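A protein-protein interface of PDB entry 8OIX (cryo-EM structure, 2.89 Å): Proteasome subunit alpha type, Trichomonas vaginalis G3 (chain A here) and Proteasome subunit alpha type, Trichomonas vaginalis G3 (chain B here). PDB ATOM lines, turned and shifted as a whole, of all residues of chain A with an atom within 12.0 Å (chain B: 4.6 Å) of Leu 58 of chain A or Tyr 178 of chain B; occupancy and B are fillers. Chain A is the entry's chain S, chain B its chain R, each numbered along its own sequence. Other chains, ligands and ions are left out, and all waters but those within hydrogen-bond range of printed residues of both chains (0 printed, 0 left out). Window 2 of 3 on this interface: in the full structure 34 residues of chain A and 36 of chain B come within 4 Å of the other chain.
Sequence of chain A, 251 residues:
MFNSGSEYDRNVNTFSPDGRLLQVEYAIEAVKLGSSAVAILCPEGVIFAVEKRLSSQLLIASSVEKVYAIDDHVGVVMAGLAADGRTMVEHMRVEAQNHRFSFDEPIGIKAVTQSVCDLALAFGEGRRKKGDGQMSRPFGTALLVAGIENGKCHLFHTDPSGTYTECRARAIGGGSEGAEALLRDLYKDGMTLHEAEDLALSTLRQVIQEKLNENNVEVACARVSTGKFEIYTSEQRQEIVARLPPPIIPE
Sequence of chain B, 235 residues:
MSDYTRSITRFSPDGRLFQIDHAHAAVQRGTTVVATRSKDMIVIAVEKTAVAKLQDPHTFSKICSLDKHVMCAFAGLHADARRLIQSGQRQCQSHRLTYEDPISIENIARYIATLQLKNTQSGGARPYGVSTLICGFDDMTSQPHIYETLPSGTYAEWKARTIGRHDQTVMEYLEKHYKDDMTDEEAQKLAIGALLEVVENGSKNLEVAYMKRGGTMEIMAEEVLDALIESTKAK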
ATOM      1  N   LYS A  52       0.770 -25.980 -33.129  1.00  0.00           N
ATOM      2  CA  LYS A  52      -0.073 -25.507 -32.039  1.00  0.00           C
ATOM      3  C   LYS A  52       0.197 -24.019 -31.854  1.00  0.00           C
ATOM      4  O   LYS A  52       1.273 -23.630 -31.389  1.00  0.00           O
ATOM      5  CB  LYS A  52       0.200 -26.285 -30.755  1.00  0.00           C
ATOM      6  CG  LYS A  52      -0.522 -27.617 -30.674  1.00  0.00           C
ATOM      7  CD  LYS A  52      -0.534 -28.156 -29.255  1.00  0.00           C
ATOM      8  CE  LYS A  52       0.874 -28.417 -28.754  1.00  0.00           C
ATOM      9  NZ  LYS A  52       0.888 -29.332 -27.580  1.00  0.00           N
ATOM     10  N   ARG A  53      -0.774 -23.189 -32.222  1.00  0.00           N
ATOM     11  CA  ARG A  53      -0.636 -21.749 -32.064  1.00  0.00           C
ATOM     12  C   ARG A  53      -0.937 -21.378 -30.618  1.00  0.00           C
ATOM     13  O   ARG A  53      -2.045 -21.615 -30.126  1.00  0.00           O
ATOM     14  CB  ARG A  53      -1.568 -21.010 -33.023  1.00  0.00           C
ATOM     15  CG  ARG A  53      -1.216 -21.195 -34.489  1.00  0.00           C
ATOM     16  CD  ARG A  53      -2.146 -20.402 -35.392  1.00  0.00           C
ATOM     17  NE  ARG A  53      -1.862 -20.639 -36.802  1.00  0.00           N
ATOM     18  CZ  ARG A  53      -2.587 -20.162 -37.805  1.00  0.00           C
ATOM     19  NH1 ARG A  53      -3.651 -19.407 -37.591  1.00  0.00           N
ATOM     20  NH2 ARG A  53      -2.235 -20.450 -39.055  1.00  0.00           N
ATOM     21  N   LEU A  54       0.048 -20.799 -29.942  1.00  0.00           N
ATOM     22  CA  LEU A  54      -0.063 -20.425 -28.537  1.00  0.00           C
ATOM     23  C   LEU A  54       0.005 -18.905 -28.446  1.00  0.00           C
ATOM     24  O   LEU A  54       1.087 -18.317 -28.533  1.00  0.00           O
ATOM     25  CB  LEU A  54       1.037 -21.087 -27.713  1.00  0.00           C
ATOM     26  CG  LEU A  54       1.092 -22.615 -27.767  1.00  0.00           C
ATOM     27  CD1 LEU A  54       2.346 -23.133 -27.081  1.00  0.00           C
ATOM     28  CD2 LEU A  54      -0.153 -23.221 -27.143  1.00  0.00           C
ATOM     29  N   SER A  55      -1.157 -18.271 -28.274  1.00  0.00           N
ATOM     30  CA  SER A  55      -1.197 -16.821 -28.129  1.00  0.00           C
ATOM     31  C   SER A  55      -0.467 -16.351 -26.879  1.00  0.00           C
ATOM     32  O   SER A  55      -0.087 -15.178 -26.799  1.00  0.00           O
ATOM     33  CB  SER A  55      -2.647 -16.333 -28.104  1.00  0.00           C
ATOM     34  OG  SER A  55      -3.355 -16.888 -27.011  1.00  0.00           O
ATOM     35  N   SER A  56      -0.264 -17.237 -25.908  1.00  0.00           N
ATOM     36  CA  SER A  56       0.463 -16.903 -24.691  1.00  0.00           C
ATOM     37  C   SER A  56       1.058 -18.178 -24.117  1.00  0.00           C
ATOM     38  O   SER A  56       0.654 -19.288 -24.469  1.00  0.00           O
ATOM     39  CB  SER A  56      -0.446 -16.228 -23.659  1.00  0.00           C
ATOM     40  OG  SER A  56      -1.149 -15.137 -24.227  1.00  0.00           O
ATOM     41  N   GLN A  57       2.036 -18.001 -23.225  1.00  0.00           N
ATOM     42  CA  GLN A  57       2.588 -19.139 -22.502  1.00  0.00           C
ATOM     43  C   GLN A  57       1.618 -19.665 -21.457  1.00  0.00           C
ATOM     44  O   GLN A  57       1.763 -20.806 -21.006  1.00  0.00           O
ATOM     45  CB  GLN A  57       3.912 -18.761 -21.836  1.00  0.00           C
ATOM     46  CG  GLN A  57       4.907 -18.064 -22.752  1.00  0.00           C
ATOM     47  CD  GLN A  57       4.754 -16.554 -22.740  1.00  0.00           C
ATOM     48  OE1 GLN A  57       3.681 -16.029 -22.441  1.00  0.00           O
ATOM     49  NE2 GLN A  57       5.832 -15.847 -23.061  1.00  0.00           N
ATOM     50  N   LEU A  58       0.633 -18.855 -21.064  1.00  0.00           N
ATOM     51  CA  LEU A  58      -0.384 -19.297 -20.120  1.00  0.00           C
ATOM     52  C   LEU A  58      -1.354 -20.286 -20.745  1.00  0.00           C
ATOM     53  O   LEU A  58      -2.027 -21.024 -20.016  1.00  0.00           O
ATOM     54  CB  LEU A  58      -1.146 -18.089 -19.583  1.00  0.00           C
ATOM     55  CG  LEU A  58      -0.244 -17.053 -18.916  1.00  0.00           C
ATOM     56  CD1 LEU A  58      -1.039 -15.846 -18.460  1.00  0.00           C
ATOM     57  CD2 LEU A  58       0.497 -17.685 -17.759  1.00  0.00           C
ATOM     58  N   LEU A  59      -1.442 -20.313 -22.071  1.00  0.00           N
ATOM     59  CA  LEU A  59      -2.307 -21.260 -22.759  1.00  0.00           C
ATOM     60  C   LEU A  59      -1.769 -22.675 -22.591  1.00  0.00           C
ATOM     61  O   LEU A  59      -0.660 -22.983 -23.042  1.00  0.00           O
ATOM     62  CB  LEU A  59      -2.409 -20.890 -24.236  1.00  0.00           C
ATOM     63  CG  LEU A  59      -3.108 -21.885 -25.159  1.00  0.00           C
ATOM     64  CD1 LEU A  59      -4.440 -22.291 -24.570  1.00  0.00           C
ATOM     65  CD2 LEU A  59      -3.295 -21.285 -26.540  1.00  0.00           C
ATOM     66  N   ILE A  60      -2.549 -23.532 -21.936  1.00  0.00           N
ATOM     67  CA  ILE A  60      -2.200 -24.940 -21.789  1.00  0.00           C
ATOM     68  C   ILE A  60      -2.197 -25.580 -23.171  1.00  0.00           C
ATOM     69  O   ILE A  60      -3.245 -25.699 -23.815  1.00  0.00           O
ATOM     70  CB  ILE A  60      -3.175 -25.659 -20.839  1.00  0.00           C
ATOM     71  CG1 ILE A  60      -3.072 -25.077 -19.430  1.00  0.00           C
ATOM     72  CG2 ILE A  60      -2.886 -27.142 -20.806  1.00  0.00           C
ATOM     73  CD1 ILE A  60      -1.777 -25.409 -18.734  1.00  0.00           C
ATOM     74  N   ALA A  61      -1.013 -25.986 -23.637  1.00  0.00           N
ATOM     75  CA  ALA A  61      -0.887 -26.529 -24.986  1.00  0.00           C
ATOM     76  C   ALA A  61      -1.709 -27.799 -25.164  1.00  0.00           C
ATOM     77  O   ALA A  61      -2.360 -27.987 -26.199  1.00  0.00           O
ATOM     78  CB  ALA A  61       0.584 -26.791 -25.307  1.00  0.00           C
ATOM     79  N   SER A  62      -1.720 -28.672 -24.153  1.00  0.00           N
ATOM     80  CA  SER A  62      -2.465 -29.921 -24.266  1.00  0.00           C
ATOM     81  C   SER A  62      -3.949 -29.680 -24.500  1.00  0.00           C
ATOM     82  O   SER A  62      -4.640 -30.572 -25.003  1.00  0.00           O
ATOM     83  CB  SER A  62      -2.261 -30.780 -23.016  1.00  0.00           C
ATOM     84  OG  SER A  62      -2.634 -30.083 -21.842  1.00  0.00           O
ATOM     85  N   SER A  63      -4.453 -28.501 -24.143  1.00  0.00           N
ATOM     86  CA  SER A  63      -5.863 -28.186 -24.302  1.00  0.00           C
ATOM     87  C   SER A  63      -6.196 -27.594 -25.663  1.00  0.00           C
ATOM     88  O   SER A  63      -7.381 -27.487 -25.996  1.00  0.00           O
ATOM     89  CB  SER A  63      -6.308 -27.214 -23.214  1.00  0.00           C
ATOM     90  OG  SER A  63      -5.892 -25.893 -23.512  1.00  0.00           O
ATOM     91  N   VAL A  64      -5.197 -27.208 -26.455  1.00  0.00           N
ATOM     92  CA  VAL A  64      -5.465 -26.712 -27.801  1.00  0.00           C
ATOM     93  C   VAL A  64      -5.058 -27.809 -28.770  1.00  0.00           C
ATOM     94  O   VAL A  64      -4.640 -27.538 -29.901  1.00  0.00           O
ATOM     95  CB  VAL A  64      -4.740 -25.388 -28.106  1.00  0.00           C
ATOM     96  CG1 VAL A  64      -5.432 -24.238 -27.404  1.00  0.00           C
ATOM     97  CG2 VAL A  64      -3.280 -25.461 -27.703  1.00  0.00           C
ATOM     98  N   GLU A  65      -5.165 -29.054 -28.309  1.00  0.00           N
ATOM     99  CA  GLU A  65      -4.790 -30.223 -29.088  1.00  0.00           C
ATOM    100  C   GLU A  65      -5.505 -30.232 -30.432  1.00  0.00           C
ATOM    101  O   GLU A  65      -6.731 -30.358 -30.498  1.00  0.00           O
ATOM    102  CB  GLU A  65      -5.089 -31.503 -28.295  1.00  0.00           C
ATOM    103  CG  GLU A  65      -6.528 -31.619 -27.793  1.00  0.00           C
ATOM    104  CD  GLU A  65      -6.735 -32.789 -26.853  1.00  0.00           C
ATOM    105  OE1 GLU A  65      -5.881 -33.001 -25.967  1.00  0.00           O
ATOM    106  OE2 GLU A  65      -7.754 -33.494 -26.999  1.00  0.00           O
ATOM    107  N   GLU A 210       7.127 -19.612 -36.550  1.00  0.00           N
ATOM    108  CA  GLU A 210       7.822 -19.632 -35.272  1.00  0.00           C
ATOM    109  C   GLU A 210       8.775 -20.816 -35.250  1.00  0.00           C
ATOM    110  O   GLU A 210       8.558 -21.814 -35.940  1.00  0.00           O
ATOM    111  CB  GLU A 210       6.838 -19.719 -34.098  1.00  0.00           C
ATOM    112  CG  GLU A 210       7.420 -19.295 -32.758  1.00  0.00           C
ATOM    113  CD  GLU A 210       6.356 -19.116 -31.693  1.00  0.00           C
ATOM    114  OE1 GLU A 210       5.226 -19.609 -31.890  1.00  0.00           O
ATOM    115  OE2 GLU A 210       6.650 -18.478 -30.659  1.00  0.00           O
ATOM    116  N   ASN A 215       6.738 -27.828 -27.406  1.00  0.00           N
ATOM    117  CA  ASN A 215       5.526 -27.302 -26.791  1.00  0.00           C
ATOM    118  C   ASN A 215       4.565 -26.674 -27.793  1.00  0.00           C
ATOM    119  O   ASN A 215       3.351 -26.692 -27.561  1.00  0.00           O
ATOM    120  CB  ASN A 215       5.886 -26.283 -25.701  1.00  0.00           C
ATOM    121  CG  ASN A 215       6.690 -25.100 -26.230  1.00  0.00           C
ATOM    122  OD1 ASN A 215       6.507 -24.653 -27.362  1.00  0.00           O
ATOM    123  ND2 ASN A 215       7.592 -24.593 -25.400  1.00  0.00           N
ATOM    124  N   ASN A 216       5.068 -26.123 -28.896  1.00  0.00           N
ATOM    125  CA  ASN A 216       4.219 -25.512 -29.911  1.00  0.00           C
ATOM    126  C   ASN A 216       3.934 -26.449 -31.080  1.00  0.00           C
ATOM    127  O   ASN A 216       3.442 -25.996 -32.118  1.00  0.00           O
ATOM    128  CB  ASN A 216       4.826 -24.189 -30.402  1.00  0.00           C
ATOM    129  CG  ASN A 216       6.052 -24.372 -31.290  1.00  0.00           C
ATOM    130  OD1 ASN A 216       6.528 -25.481 -31.514  1.00  0.00           O
ATOM    131  ND2 ASN A 216       6.566 -23.261 -31.802  1.00  0.00           N
ATOM    132  N   GLU B 157      -7.809 -24.555 -22.195  1.00  0.00           N
ATOM    133  CA  GLU B 157      -7.396 -24.414 -20.805  1.00  0.00           C
ATOM    134  C   GLU B 157      -6.253 -23.416 -20.688  1.00  0.00           C
ATOM    135  O   GLU B 157      -5.385 -23.334 -21.560  1.00  0.00           O
ATOM    136  CB  GLU B 157      -6.972 -25.761 -20.224  1.00  0.00           C
ATOM    137  CG  GLU B 157      -6.799 -25.774 -18.718  1.00  0.00           C
ATOM    138  CD  GLU B 157      -6.368 -27.129 -18.201  1.00  0.00           C
ATOM    139  OE1 GLU B 157      -6.522 -28.121 -18.942  1.00  0.00           O
ATOM    140  OE2 GLU B 157      -5.875 -27.204 -17.055  1.00  0.00           O
ATOM    141  N   TRP B 158      -6.257 -22.654 -19.598  1.00  0.00           N
ATOM    142  CA  TRP B 158      -5.247 -21.637 -19.363  1.00  0.00           C
ATOM    143  C   TRP B 158      -4.747 -21.732 -17.931  1.00  0.00           C
ATOM    144  O   TRP B 158      -5.470 -22.164 -17.030  1.00  0.00           O
ATOM    145  CB  TRP B 158      -5.788 -20.225 -19.615  1.00  0.00           C
ATOM    146  CG  TRP B 158      -6.076 -19.920 -21.048  1.00  0.00           C
ATOM    147  CD1 TRP B 158      -7.140 -20.349 -21.777  1.00  0.00           C
ATOM    148  CD2 TRP B 158      -5.297 -19.096 -21.921  1.00  0.00           C
ATOM    149  NE1 TRP B 158      -7.070 -19.856 -23.055  1.00  0.00           N
ATOM    150  CE2 TRP B 158      -5.945 -19.082 -23.169  1.00  0.00           C
ATOM    151  CE3 TRP B 158      -4.111 -18.373 -21.769  1.00  0.00           C
ATOM    152  CZ2 TRP B 158      -5.449 -18.375 -24.259  1.00  0.00           C
ATOM    153  CZ3 TRP B 158      -3.619 -17.673 -22.853  1.00  0.00           C
ATOM    154  CH2 TRP B 158      -4.287 -17.678 -24.082  1.00  0.00           C
ATOM    155  N   LYS B 159      -3.492 -21.328 -17.736  1.00  0.00           N
ATOM    156  CA  LYS B 159      -2.971 -21.134 -16.391  1.00  0.00           C
ATOM    157  C   LYS B 159      -3.510 -19.852 -15.775  1.00  0.00           C
ATOM    158  O   LYS B 159      -3.731 -19.793 -14.560  1.00  0.00           O
ATOM    159  CB  LYS B 159      -1.444 -21.111 -16.422  1.00  0.00           C
ATOM    160  CG  LYS B 159      -0.825 -22.356 -17.034  1.00  0.00           C
ATOM    161  CD  LYS B 159       0.684 -22.235 -17.143  1.00  0.00           C
ATOM    162  CE  LYS B 159       1.301 -23.513 -17.684  1.00  0.00           C
ATOM    163  NZ  LYS B 159       2.787 -23.440 -17.723  1.00  0.00           N
ATOM    164  N   ALA B 160      -3.726 -18.829 -16.597  1.00  0.00           N
ATOM    165  CA  ALA B 160      -4.380 -17.596 -16.170  1.00  0.00           C
ATOM    166  C   ALA B 160      -4.909 -16.911 -17.418  1.00  0.00           C
ATOM    167  O   ALA B 160      -4.133 -16.592 -18.322  1.00  0.00           O
ATOM    168  CB  ALA B 160      -3.415 -16.686 -15.415  1.00  0.00           C
ATOM    169  N   MET B 171      -4.221  -9.621 -20.057  1.00  0.00           N
ATOM    170  CA  MET B 171      -3.429 -10.761 -20.508  1.00  0.00           C
ATOM    171  C   MET B 171      -1.940 -10.474 -20.390  1.00  0.00           C
ATOM    172  O   MET B 171      -1.167 -11.338 -19.964  1.00  0.00           O
ATOM    173  CB  MET B 171      -3.774 -11.125 -21.954  1.00  0.00           C
ATOM    174  CG  MET B 171      -4.798 -12.238 -22.115  1.00  0.00           C
ATOM    175  SD  MET B 171      -4.462 -13.711 -21.124  1.00  0.00           S
ATOM    176  CE  MET B 171      -2.770 -14.079 -21.580  1.00  0.00           C
ATOM    177  N   LEU B 174      -1.039 -10.714 -16.747  1.00  0.00           N
ATOM    178  CA  LEU B 174      -0.976 -12.109 -16.326  1.00  0.00           C
ATOM    179  C   LEU B 174       0.303 -12.772 -16.816  1.00  0.00           C
ATOM    180  O   LEU B 174       0.983 -13.470 -16.059  1.00  0.00           O
ATOM    181  CB  LEU B 174      -2.202 -12.867 -16.833  1.00  0.00           C
ATOM    182  CG  LEU B 174      -3.557 -12.520 -16.219  1.00  0.00           C
ATOM    183  CD1 LEU B 174      -4.670 -13.214 -16.981  1.00  0.00           C
ATOM    184  CD2 LEU B 174      -3.585 -12.910 -14.752  1.00  0.00           C
ATOM    185  N   GLU B 175       0.653 -12.551 -18.086  1.00  0.00           N
ATOM    186  CA  GLU B 175       1.866 -13.148 -18.634  1.00  0.00           C
ATOM    187  C   GLU B 175       3.099 -12.668 -17.883  1.00  0.00           C
ATOM    188  O   GLU B 175       4.011 -13.453 -17.603  1.00  0.00           O
ATOM    189  CB  GLU B 175       1.991 -12.817 -20.121  1.00  0.00           C
ATOM    190  CG  GLU B 175       0.907 -13.409 -21.000  1.00  0.00           C
ATOM    191  CD  GLU B 175       0.971 -12.883 -22.421  1.00  0.00           C
ATOM    192  OE1 GLU B 175       1.949 -12.180 -22.751  1.00  0.00           O
ATOM    193  OE2 GLU B 175       0.039 -13.158 -23.205  1.00  0.00           O
ATOM    194  N   LYS B 176       3.146 -11.376 -17.554  1.00  0.00           N
ATOM    195  CA  LYS B 176       4.304 -10.835 -16.852  1.00  0.00           C
ATOM    196  C   LYS B 176       4.398 -11.373 -15.427  1.00  0.00           C
ATOM    197  O   LYS B 176       5.464 -11.825 -14.995  1.00  0.00           O
ATOM    198  CB  LYS B 176       4.251  -9.307 -16.856  1.00  0.00           C
ATOM    199  CG  LYS B 176       5.480  -8.645 -16.257  1.00  0.00           C
ATOM    200  CD  LYS B 176       5.677  -7.242 -16.809  1.00  0.00           C
ATOM    201  CE  LYS B 176       4.565  -6.305 -16.371  1.00  0.00           C
ATOM    202  NZ  LYS B 176       4.750  -4.937 -16.930  1.00  0.00           N
ATOM    203  N   HIS B 177       3.293 -11.340 -14.682  1.00  0.00           N
ATOM    204  CA  HIS B 177       3.309 -11.622 -13.253  1.00  0.00           C
ATOM    205  C   HIS B 177       2.863 -13.041 -12.907  1.00  0.00           C
ATOM    206  O   HIS B 177       2.455 -13.287 -11.767  1.00  0.00           O
ATOM    207  CB  HIS B 177       2.437 -10.613 -12.504  1.00  0.00           C
ATOM    208  CG  HIS B 177       2.857  -9.189 -12.692  1.00  0.00           C
ATOM    209  ND1 HIS B 177       2.256  -8.349 -13.604  1.00  0.00           N
ATOM    210  CD2 HIS B 177       3.815  -8.455 -12.080  1.00  0.00           C
ATOM    211  CE1 HIS B 177       2.825  -7.158 -13.545  1.00  0.00           C
ATOM    212  NE2 HIS B 177       3.777  -7.197 -12.630  1.00  0.00           N
ATOM    213  N   TYR B 178       2.926 -13.976 -13.851  1.00  0.00           N
ATOM    214  CA  TYR B 178       2.549 -15.356 -13.567  1.00  0.00           C
ATOM    215  C   TYR B 178       3.757 -16.151 -13.088  1.00  0.00           C
ATOM    216  O   TYR B 178       4.843 -16.060 -13.670  1.00  0.00           O
ATOM    217  CB  TYR B 178       1.933 -16.034 -14.791  1.00  0.00           C
ATOM    218  CG  TYR B 178       1.623 -17.501 -14.578  1.00  0.00           C
ATOM    219  CD1 TYR B 178       0.410 -17.897 -14.035  1.00  0.00           C
ATOM    220  CD2 TYR B 178       2.531 -18.488 -14.943  1.00  0.00           C
ATOM    221  CE1 TYR B 178       0.116 -19.231 -13.839  1.00  0.00           C
ATOM    222  CE2 TYR B 178       2.243 -19.827 -14.755  1.00  0.00           C
ATOM    223  CZ  TYR B 178       1.035 -20.191 -14.202  1.00  0.00           C
ATOM    224  OH  TYR B 178       0.743 -21.521 -14.009  1.00  0.00           O
ATOM    225  N   LYS B 179       3.555 -16.927 -12.030  1.00  0.00           N
ATOM    226  CA  LYS B 179       4.553 -17.844 -11.501  1.00  0.00           C
ATOM    227  C   LYS B 179       4.110 -19.271 -11.790  1.00  0.00           C
ATOM    228  O   LYS B 179       2.913 -19.568 -11.793  1.00  0.00           O
ATOM    229  CB  LYS B 179       4.748 -17.642  -9.996  1.00  0.00           C
ATOM    230  CG  LYS B 179       5.095 -16.217  -9.604  1.00  0.00           C
ATOM    231  CD  LYS B 179       5.040 -16.029  -8.098  1.00  0.00           C
ATOM    232  CE  LYS B 179       6.114 -16.850  -7.405  1.00  0.00           C
ATOM    233  NZ  LYS B 179       7.481 -16.473  -7.860  1.00  0.00           N
ATOM    234  N   ASP B 180       5.074 -20.149 -12.069  1.00  0.00           N
ATOM    235  CA  ASP B 180       4.719 -21.510 -12.458  1.00  0.00           C
ATOM    236  C   ASP B 180       4.060 -22.268 -11.310  1.00  0.00           C
ATOM    237  O   ASP B 180       3.145 -23.067 -11.542  1.00  0.00           O
ATOM    238  CB  ASP B 180       5.967 -22.249 -12.948  1.00  0.00           C
ATOM    239  CG  ASP B 180       5.641 -23.499 -13.756  1.00  0.00           C
ATOM    240  OD1 ASP B 180       4.511 -24.020 -13.652  1.00  0.00           O
ATOM    241  OD2 ASP B 180       6.527 -23.963 -14.503  1.00  0.00           O
ATOM    242  N   MET B 182       2.588 -20.947  -8.205  1.00  0.00           N
ATOM    243  CA  MET B 182       2.058 -19.987  -7.246  1.00  0.00           C
ATOM    244  C   MET B 182       1.325 -20.695  -6.113  1.00  0.00           C
ATOM    245  O   MET B 182       0.741 -21.767  -6.290  1.00  0.00           O
ATOM    246  CB  MET B 182       1.096 -19.006  -7.917  1.00  0.00           C
ATOM    247  CG  MET B 182       1.357 -18.753  -9.376  1.00  0.00           C
ATOM    248  SD  MET B 182       0.370 -17.397 -10.036  1.00  0.00           S
ATOM    249  CE  MET B 182       0.962 -16.033  -9.042  1.00  0.00           C
ATOM    250  N   LEU B 190      -2.244 -12.299  -8.036  1.00  0.00           N
ATOM    251  CA  LEU B 190      -2.110 -12.133  -9.479  1.00  0.00           C
ATOM    252  C   LEU B 190      -3.433 -11.718 -10.108  1.00  0.00           C
ATOM    253  O   LEU B 190      -3.488 -10.756 -10.882  1.00  0.00           O
ATOM    254  CB  LEU B 190      -1.593 -13.424 -10.114  1.00  0.00           C
ATOM    255  CG  LEU B 190      -1.537 -13.465 -11.645  1.00  0.00           C
ATOM    256  CD1 LEU B 190      -0.852 -12.227 -12.210  1.00  0.00           C
ATOM    257  CD2 LEU B 190      -0.835 -14.722 -12.124  1.00  0.00           C
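O of Glu 157 of chain B lies within hydrogen-bond range of N of Ile 60 of chain A (2.9 Å). The backbone NH of Glu 157 of chain B sits at hydrogen-bond distance from the side-chain hydroxyl of Ser 63 of chain A (2.7 Å). The backbone NH (N) of Lys 159 of chain B sits at hydrogen-bond distance from the backbone carbonyl oxygen (O) of Leu 58 of chain A (2.7 Å). The side-chain carboxylate (OE2) of Glu 175 of chain B is in hydrogen-bond range of the side-chain hydroxyl (OG) of Ser 56 of chain A (2.5 Å).
The backbone carbonyl oxygen (O) of Ile 60 of chain A sits at hydrogen-bond distance from the side-chain hydroxyl (OG) of Ser 63 of chain A, 2.7 Å away.
Among the printed residues, pairs that only touch across the chains: Ser 55 of chain A with Trp 158 of chain B (3.2 Å), Ser 56 of chain A with Trp 158 of chain B (3.6 Å), Ser 56 of chain A with Met 171 of chain B (3.3 Å), Leu 58 of chain A with Trp 158 of chain B (3.3 Å), Leu 58 of chain A with Ala 160 of chain B (3.2 Å), Leu 58 of chain A with Met 171 of chain B (3.98 Å), Leu 58 of chain A with Leu 174 of chain B (3.6 Å), Leu 58 of chain A with Glu 175 of chain B (3.7 Å), Leu 58 of chain A with Tyr 178 of chain B (3.4 Å), Leu 59 of chain A with Glu 157 of chain B (3.3 Å), Leu 59 of chain A with Trp 158 of chain B (3.3 Å) and Ile 60 of chain A with Lys 159 of chain B (3.6 Å).
Of the printed residues of chain B, Leu 59 of chain A touches Glu 157 and Trp 158. Of the printed residues of chain A, Glu 157 of chain B touches Leu 59 (3.3 Å), Ile 60 (2.9 Å) and Ser 63 (2.7 Å). Of the printed residues of chain A, Trp 158 of chain B touches Ser 55 (3.2 Å), Ser 56 (3.6 Å), Leu 58 (3.3 Å) and Leu 59 (3.3 Å). Lys 159 of chain B touches just these residues of chain A: Leu 58 and Ile 60. Of the printed residues of chain A, Met 171 of chain B touches Ser 56 (3.3 Å) and Leu 58 (3.98 Å). Of chain A, only Ser 56 and Leu 58 come within 4 Å of Glu 175 of chain B. No residue of chain A comes within 4 Å of His 177 of chain B. Of chain A, only Leu 58 (3.4 Å) comes within 4 Å of Tyr 178 of chain B. No residue of chain A comes within 4 Å of Lys 179 of chain B. Asp 180 of chain B touches none of the printed residues of chain A. No residue of chain A comes within 4 Å of Leu 190 of chain B. The nearest residue of chain A that does not touch Tyr 178 of chain B is Gln 57 of chain A (6.3 Å).
Of the 14 printed residues of chain B, 8 touch a printed residue of chain A. Hydrophobic or aromatic side chains of chain B within 4 Å of the printed part of chain A: Trp 158, Ala 160, Met 171, Leu 174 and Tyr 178. Of the 17 printed residues of chain A, 6 touch a printed residue of chain B. Among the printed residues, 16 pairs touch across the chains. Among the printed residues, no Asp or Glu carboxylate lies within 4 Å of a Lys or Arg side-chain nitrogen of the other chain.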
